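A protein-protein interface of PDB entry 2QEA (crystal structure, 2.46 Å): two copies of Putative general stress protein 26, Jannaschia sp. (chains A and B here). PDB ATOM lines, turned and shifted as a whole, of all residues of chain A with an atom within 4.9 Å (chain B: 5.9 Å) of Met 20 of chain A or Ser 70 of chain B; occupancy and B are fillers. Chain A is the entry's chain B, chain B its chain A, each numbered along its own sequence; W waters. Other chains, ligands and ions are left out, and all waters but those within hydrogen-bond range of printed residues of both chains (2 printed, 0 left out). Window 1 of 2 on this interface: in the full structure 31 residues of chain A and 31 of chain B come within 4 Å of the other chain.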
ATOM      1  N   SER A  18      28.058  33.183 -25.073  1.00  0.00           N
ATOM      2  CA  SER A  18      27.906  31.727 -24.934  1.00  0.00           C
ATOM      3  C   SER A  18      27.971  30.933 -26.240  1.00  0.00           C
ATOM      4  O   SER A  18      27.697  31.451 -27.322  1.00  0.00           O
ATOM      5  CB  SER A  18      26.568  31.415 -24.264  1.00  0.00           C
ATOM      6  OG  SER A  18      26.453  32.071 -23.014  1.00  0.00           O
ATOM      7  N   GLY A  19      28.318  29.655 -26.102  1.00  0.00           N
ATOM      8  CA  GLY A  19      28.388  28.701 -27.214  1.00  0.00           C
ATOM      9  C   GLY A  19      28.281  27.278 -26.693  1.00  0.00           C
ATOM     10  O   GLY A  19      28.491  27.042 -25.504  1.00  0.00           O
ATOM     11  N   MET A  20      27.978  26.336 -27.584  1.00  0.00           N
ATOM     12  CA  MET A  20      27.773  24.923 -27.227  1.00  0.00           C
ATOM     13  C   MET A  20      28.987  24.084 -27.643  1.00  0.00           C
ATOM     14  O   MET A  20      29.203  23.868 -28.832  1.00  0.00           O
ATOM     15  CB  MET A  20      26.485  24.415 -27.879  1.00  0.00           C
ATOM     16  CG  MET A  20      25.240  25.208 -27.484  1.00  0.00           C
ATOM     17  SD  MET A  20      24.722  24.972 -25.627  1.00  0.00           S
ATOM     18  CE  MET A  20      24.082  23.130 -25.711  1.00  0.00           C
ATOM     19  N   LEU A  21      29.753  23.611 -26.651  1.00  0.00           N
ATOM     20  CA  LEU A  21      31.007  22.865 -26.854  1.00  0.00           C
ATOM     21  C   LEU A  21      30.901  21.389 -26.473  1.00  0.00           C
ATOM     22  O   LEU A  21      30.138  21.023 -25.577  1.00  0.00           O
ATOM     23  CB  LEU A  21      32.111  23.510 -26.008  1.00  0.00           C
ATOM     24  CG  LEU A  21      33.566  23.053 -26.155  1.00  0.00           C
ATOM     25  CD1 LEU A  21      34.073  23.308 -27.562  1.00  0.00           C
ATOM     26  CD2 LEU A  21      34.437  23.778 -25.134  1.00  0.00           C
ATOM     27  N   GLY A  22      31.697  20.557 -27.144  1.00  0.00           N
ATOM     28  CA  GLY A  22      31.733  19.118 -26.875  1.00  0.00           C
ATOM     29  C   GLY A  22      32.787  18.356 -27.661  1.00  0.00           C
ATOM     30  O   GLY A  22      33.235  18.815 -28.712  1.00  0.00           O
ATOM     31  N   LEU A  29      26.491  18.294 -26.421  1.00  0.00           N
ATOM     32  CA  LEU A  29      27.062  19.639 -26.310  1.00  0.00           C
ATOM     33  C   LEU A  29      26.510  20.337 -25.058  1.00  0.00           C
ATOM     34  O   LEU A  29      25.353  20.115 -24.685  1.00  0.00           O
ATOM     35  CB  LEU A  29      26.744  20.480 -27.551  1.00  0.00           C
ATOM     36  CG  LEU A  29      27.208  19.968 -28.920  1.00  0.00           C
ATOM     37  CD1 LEU A  29      26.637  20.837 -30.035  1.00  0.00           C
ATOM     38  CD2 LEU A  29      28.723  19.918 -29.003  1.00  0.00           C
ATOM     39  N   ILE A  30      27.348  21.156 -24.415  1.00  0.00           N
ATOM     40  CA  ILE A  30      26.978  21.910 -23.199  1.00  0.00           C
ATOM     41  C   ILE A  30      27.363  23.392 -23.343  1.00  0.00           C
ATOM     42  O   ILE A  30      28.313  23.698 -24.068  1.00  0.00           O
ATOM     43  CB  ILE A  30      27.622  21.295 -21.916  1.00  0.00           C
ATOM     44  CG1 ILE A  30      29.160  21.306 -21.973  1.00  0.00           C
ATOM     45  CG2 ILE A  30      27.114  19.869 -21.711  1.00  0.00           C
ATOM     46  CD1 ILE A  30      29.822  20.792 -20.698  1.00  0.00           C
ATOM     47  N   PRO A  31      26.643  24.308 -22.648  1.00  0.00           N
ATOM     48  CA  PRO A  31      26.975  25.738 -22.756  1.00  0.00           C
ATOM     49  C   PRO A  31      28.319  26.116 -22.105  1.00  0.00           C
ATOM     50  O   PRO A  31      28.616  25.653 -21.000  1.00  0.00           O
ATOM     51  CB  PRO A  31      25.799  26.429 -22.051  1.00  0.00           C
ATOM     52  CG  PRO A  31      25.279  25.426 -21.114  1.00  0.00           C
ATOM     53  CD  PRO A  31      25.488  24.092 -21.754  1.00  0.00           C
ATOM     54  N   GLN A  66      33.623  19.682 -31.371  1.00  0.00           N
ATOM     55  CA  GLN A  66      32.622  20.504 -32.036  1.00  0.00           C
ATOM     56  C   GLN A  66      32.305  21.721 -31.168  1.00  0.00           C
ATOM     57  O   GLN A  66      32.256  21.613 -29.939  1.00  0.00           O
ATOM     58  CB  GLN A  66      31.344  19.694 -32.259  1.00  0.00           C
ATOM     59  CG  GLN A  66      30.263  20.410 -33.085  1.00  0.00           C
ATOM     60  CD  GLN A  66      29.032  19.555 -33.336  1.00  0.00           C
ATOM     61  OE1 GLN A  66      28.758  18.596 -32.613  1.00  0.00           O
ATOM     62  NE2 GLN A  66      28.271  19.916 -34.365  1.00  0.00           N
ATOM     63  N   PHE A  67      32.105  22.868 -31.817  1.00  0.00           N
ATOM     64  CA  PHE A  67      31.690  24.105 -31.142  1.00  0.00           C
ATOM     65  C   PHE A  67      30.623  24.769 -32.009  1.00  0.00           C
ATOM     66  O   PHE A  67      30.869  25.033 -33.188  1.00  0.00           O
ATOM     67  CB  PHE A  67      32.875  25.037 -30.883  1.00  0.00           C
ATOM     68  CG  PHE A  67      32.512  26.279 -30.105  1.00  0.00           C
ATOM     69  CD1 PHE A  67      32.002  26.176 -28.803  1.00  0.00           C
ATOM     70  CD2 PHE A  67      32.695  27.553 -30.656  1.00  0.00           C
ATOM     71  CE1 PHE A  67      31.650  27.321 -28.072  1.00  0.00           C
ATOM     72  CE2 PHE A  67      32.362  28.709 -29.930  1.00  0.00           C
ATOM     73  CZ  PHE A  67      31.841  28.592 -28.632  1.00  0.00           C
ATOM     74  N   VAL A  68      29.447  25.007 -31.422  1.00  0.00           N
ATOM     75  CA  VAL A  68      28.301  25.595 -32.115  1.00  0.00           C
ATOM     76  C   VAL A  68      27.951  26.956 -31.508  1.00  0.00           C
ATOM     77  O   VAL A  68      27.876  27.088 -30.282  1.00  0.00           O
ATOM     78  CB  VAL A  68      27.078  24.650 -32.063  1.00  0.00           C
ATOM     79  CG1 VAL A  68      25.868  25.277 -32.743  1.00  0.00           C
ATOM     80  CG2 VAL A  68      27.413  23.309 -32.716  1.00  0.00           C
ATOM     81  N   SER A  70      25.180  30.326 -31.884  1.00  0.00           N
ATOM     82  CA  SER A  70      23.877  30.794 -32.364  1.00  0.00           C
ATOM     83  C   SER A  70      23.528  32.038 -31.550  1.00  0.00           C
ATOM     84  O   SER A  70      22.844  31.943 -30.532  1.00  0.00           O
ATOM     85  CB  SER A  70      22.823  29.690 -32.218  1.00  0.00           C
ATOM     86  OG  SER A  70      21.547  30.126 -32.661  1.00  0.00           O
ATOM     87  N   VAL B  16      12.716  32.075 -28.126  1.00  0.00           N
ATOM     88  CA  VAL B  16      13.999  31.813 -28.794  1.00  0.00           C
ATOM     89  C   VAL B  16      13.791  32.043 -30.300  1.00  0.00           C
ATOM     90  O   VAL B  16      13.056  31.295 -30.948  1.00  0.00           O
ATOM     91  CB  VAL B  16      14.511  30.374 -28.514  1.00  0.00           C
ATOM     92  CG1 VAL B  16      15.843  30.128 -29.190  1.00  0.00           C
ATOM     93  CG2 VAL B  16      14.644  30.137 -27.007  1.00  0.00           C
ATOM     94  N   SER B  18      16.153  31.962 -32.803  1.00  0.00           N
ATOM     95  CA  SER B  18      16.979  31.093 -33.650  1.00  0.00           C
ATOM     96  C   SER B  18      17.458  29.814 -32.964  1.00  0.00           C
ATOM     97  O   SER B  18      17.535  29.730 -31.736  1.00  0.00           O
ATOM     98  CB  SER B  18      18.206  31.864 -34.145  1.00  0.00           C
ATOM     99  OG  SER B  18      17.829  33.034 -34.851  1.00  0.00           O
ATOM    100  N   VAL B  68      20.071  22.262 -31.820  1.00  0.00           N
ATOM    101  CA  VAL B  68      20.861  22.893 -30.768  1.00  0.00           C
ATOM    102  C   VAL B  68      20.345  24.314 -30.534  1.00  0.00           C
ATOM    103  O   VAL B  68      20.123  25.056 -31.496  1.00  0.00           O
ATOM    104  CB  VAL B  68      22.359  22.908 -31.142  1.00  0.00           C
ATOM    105  CG1 VAL B  68      23.191  23.579 -30.060  1.00  0.00           C
ATOM    106  CG2 VAL B  68      22.857  21.489 -31.375  1.00  0.00           C
ATOM    107  N   VAL B  69      20.155  24.669 -29.260  1.00  0.00           N
ATOM    108  CA  VAL B  69      19.694  25.997 -28.835  1.00  0.00           C
ATOM    109  C   VAL B  69      20.720  26.598 -27.864  1.00  0.00           C
ATOM    110  O   VAL B  69      21.298  25.880 -27.043  1.00  0.00           O
ATOM    111  CB  VAL B  69      18.302  25.919 -28.141  1.00  0.00           C
ATOM    112  CG1 VAL B  69      17.834  27.301 -27.659  1.00  0.00           C
ATOM    113  CG2 VAL B  69      17.271  25.323 -29.080  1.00  0.00           C
ATOM    114  N   SER B  70      20.954  27.906 -27.995  1.00  0.00           N
ATOM    115  CA  SER B  70      21.847  28.668 -27.111  1.00  0.00           C
ATOM    116  C   SER B  70      21.368  30.120 -27.137  1.00  0.00           C
ATOM    117  O   SER B  70      21.648  30.840 -28.093  1.00  0.00           O
ATOM    118  CB  SER B  70      23.305  28.546 -27.565  1.00  0.00           C
ATOM    119  OG  SER B  70      24.179  29.274 -26.712  1.00  0.00           O
ATOM    120  N   ASP B  71      20.618  30.519 -26.109  1.00  0.00           N
ATOM    121  CA  ASP B  71      20.001  31.851 -26.027  1.00  0.00           C
ATOM    122  C   ASP B  71      20.265  32.480 -24.649  1.00  0.00           C
ATOM    123  O   ASP B  71      19.742  32.002 -23.637  1.00  0.00           O
ATOM    124  CB  ASP B  71      18.496  31.700 -26.306  1.00  0.00           C
ATOM    125  CG  ASP B  71      17.799  33.024 -26.605  1.00  0.00           C
ATOM    126  OD1 ASP B  71      17.824  33.944 -25.759  1.00  0.00           O
ATOM    127  OD2 ASP B  71      17.173  33.123 -27.683  1.00  0.00           O
ATOM    128  N   ASP B  72      21.073  33.545 -24.627  1.00  0.00           N
ATOM    129  CA  ASP B  72      21.417  34.274 -23.391  1.00  0.00           C
ATOM    130  C   ASP B  72      20.251  35.092 -22.829  1.00  0.00           C
ATOM    131  O   ASP B  72      20.096  35.172 -21.606  1.00  0.00           O
ATOM    132  CB  ASP B  72      22.633  35.200 -23.603  1.00  0.00           C
ATOM    133  CG  ASP B  72      23.914  34.443 -23.955  1.00  0.00           C
ATOM    134  OD1 ASP B  72      24.098  33.286 -23.530  1.00  0.00           O
ATOM    135  OD2 ASP B  72      24.766  35.032 -24.649  1.00  0.00           O
ATOM    136  N   LEU B  76      18.269  29.697 -22.046  1.00  0.00           N
ATOM    137  CA  LEU B  76      17.901  28.343 -22.453  1.00  0.00           C
ATOM    138  C   LEU B  76      19.003  27.826 -23.364  1.00  0.00           C
ATOM    139  O   LEU B  76      19.274  28.421 -24.410  1.00  0.00           O
ATOM    140  CB  LEU B  76      16.564  28.339 -23.200  1.00  0.00           C
ATOM    141  CG  LEU B  76      16.019  26.986 -23.685  1.00  0.00           C
ATOM    142  CD1 LEU B  76      15.835  26.006 -22.530  1.00  0.00           C
ATOM    143  CD2 LEU B  76      14.713  27.185 -24.427  1.00  0.00           C
ATOM    144  N   TYR B  77      19.642  26.735 -22.942  1.00  0.00           N
ATOM    145  CA  TYR B  77      20.715  26.078 -23.691  1.00  0.00           C
ATOM    146  C   TYR B  77      20.321  24.609 -23.765  1.00  0.00           C
ATOM    147  O   TYR B  77      19.953  24.027 -22.739  1.00  0.00           O
ATOM    148  CB  TYR B  77      22.062  26.267 -22.986  1.00  0.00           C
ATOM    149  CG  TYR B  77      22.346  27.707 -22.613  1.00  0.00           C
ATOM    150  CD1 TYR B  77      22.994  28.570 -23.503  1.00  0.00           C
ATOM    151  CD2 TYR B  77      21.934  28.222 -21.373  1.00  0.00           C
ATOM    152  CE1 TYR B  77      23.242  29.915 -23.162  1.00  0.00           C
ATOM    153  CE2 TYR B  77      22.174  29.561 -21.023  1.00  0.00           C
ATOM    154  CZ  TYR B  77      22.828  30.401 -21.921  1.00  0.00           C
ATOM    155  OH  TYR B  77      23.066  31.712 -21.578  1.00  0.00           O
ATOM    156  N   ALA B  78      20.369  24.019 -24.960  1.00  0.00           N
ATOM    157  CA  ALA B  78      19.941  22.629 -25.141  1.00  0.00           C
ATOM    158  C   ALA B  78      20.476  21.976 -26.407  1.00  0.00           C
ATOM    159  O   ALA B  78      20.436  22.587 -27.468  1.00  0.00           O
ATOM    160  CB  ALA B  78      18.416  22.564 -25.153  1.00  0.00           C
ATOM    161  N   ASP B  79      20.994  20.754 -26.270  1.00  0.00           N
ATOM    162  CA  ASP B  79      21.426  19.923 -27.391  1.00  0.00           C
ATOM    163  C   ASP B  79      20.388  18.800 -27.398  1.00  0.00           C
ATOM    164  O   ASP B  79      20.383  17.969 -26.489  1.00  0.00           O
ATOM    165  CB  ASP B  79      22.851  19.388 -27.178  1.00  0.00           C
ATOM    166  CG  ASP B  79      23.360  18.536 -28.346  1.00  0.00           C
ATOM    167  OD1 ASP B  79      22.690  18.435 -29.398  1.00  0.00           O
ATOM    168  OD2 ASP B  79      24.459  17.959 -28.215  1.00  0.00           O
ATOM    169  N   GLU B 125      20.350  17.255 -23.405  1.00  0.00           N
ATOM    170  CA  GLU B 125      20.973  17.835 -22.216  1.00  0.00           C
ATOM    171  C   GLU B 125      20.608  19.314 -22.250  1.00  0.00           C
ATOM    172  O   GLU B 125      21.047  20.032 -23.151  1.00  0.00           O
ATOM    173  CB  GLU B 125      22.486  17.613 -22.190  1.00  0.00           C
ATOM    174  CG  GLU B 125      23.109  17.962 -20.829  1.00  0.00           C
ATOM    175  CD  GLU B 125      24.557  17.506 -20.648  1.00  0.00           C
ATOM    176  OE1 GLU B 125      25.091  16.745 -21.488  1.00  0.00           O
ATOM    177  OE2 GLU B 125      25.164  17.905 -19.627  1.00  0.00           O
HETATM  178  O   HOH W   1      19.857  29.394 -30.264  1.00  0.00           O
HETATM  179  O   HOH W   2      25.539  30.469 -29.029  1.00  0.00           O
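Ser 70 of chain A touches its own counterpart, Ser 70 of chain B.
Tyr 77 of chain B touches Ser 18 of chain A. CG of Met 20 of chain A touches CG1 of Val 68 of chain B, at 3.7 Å. Val 69 of chain B touches Met 20 of chain A. Met 20 of chain A touches Ser 70 of chain B (CG to CB, 3.9 Å). Met 20 of chain A touches Tyr 77 of chain B. Ala 78 of chain B touches Met 20 of chain A (C to CE, 3.8 Å). Asp 79 of chain B touches Met 20 of chain A. Ile 30 of chain A touches Glu 125 of chain B. Tyr 77 of chain B touches Pro 31 of chain A.
Met 20 of chain A touches just these residues of chain B: Val 68 (3.7 Å), Val 69 (3.8 Å), Ser 70 (3.9 Å), Tyr 77 (3.97 Å), Ala 78 (3.8 Å) and Asp 79 (3.9 Å). Of the printed residues of chain B, Pro 31 of chain A touches Tyr 77. Gln 66 of chain A touches none of the printed residues of chain B. Of chain A, only Met 20 and Ser 70 come within 4 Å of Ser 70 of chain B. Of the printed residues of chain A, Asp 72 of chain B touches Ser 18 (2.7 Å). Leu 76 of chain B touches none of the printed residues of chain A. Of the printed residues of chain A, Glu 125 of chain B touches Ile 30 (3.5 Å).
Water W1 lies within hydrogen-bond range of O of Ser 18 of chain B (2.8 Å), N of Ser 70 of chain B (2.9 Å) and OG of Ser 70 of chain A (3.0 Å). Water W2 lies within hydrogen-bond range of N of Ser 70 of chain A (2.9 Å), O of Ser 18 of chain A (2.9 Å) and OG of Ser 70 of chain B (2.9 Å).
OG of Ser 18 of chain A is in hydrogen-bond range of OD1 of Asp 72 of chain B. OD2 of Asp 79 of chain B sits at hydrogen-bond distance from N of Leu 29 of chain A (2.7 Å). The backbone carbonyl oxygen (O) of Ser 70 of chain A lies close to the backbone carbonyl oxygen (O) of Ser 70 of chain B (2.9 Å).
N of Val 69 of chain B sits at hydrogen-bond distance from O of Ala 78 of chain B, at 2.8 Å. The side-chain carboxylate (OD1) of Asp 72 of chain B is in hydrogen-bond range of the side-chain hydroxyl (OH) of Tyr 77 of chain B, at 2.7 Å. The backbone carbonyl oxygen (O) of Asp 79 of chain B lies within hydrogen-bond range of the backbone NH (N) of Glu 125 of chain B (3.2 Å). N of Met 20 of chain A sits at hydrogen-bond distance from O of Val 68 of chain A (2.8 Å). N of Leu 21 of chain A sits at hydrogen-bond distance from O of Ile 30 of chain A (3.0 Å).
Of the 12 printed residues of chain B, 8 touch a printed residue of chain A. Printed residues of chain B that touch a printed residue of chain A: Val 68, Val 69, Ser 70, Asp 72, Tyr 77, Ala 78, Asp 79 and Glu 125. Hydrophobic or aromatic side chains of chain B within 4 Å of the printed part of chain A: Val 68 and Tyr 77. Along chain B the printed residues that touch a printed residue of chain A span positions 68 to 125. Among the printed residues, no Asp or Glu carboxylate lies within 4 Å of a Lys or Arg side-chain nitrogen of the other chain.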
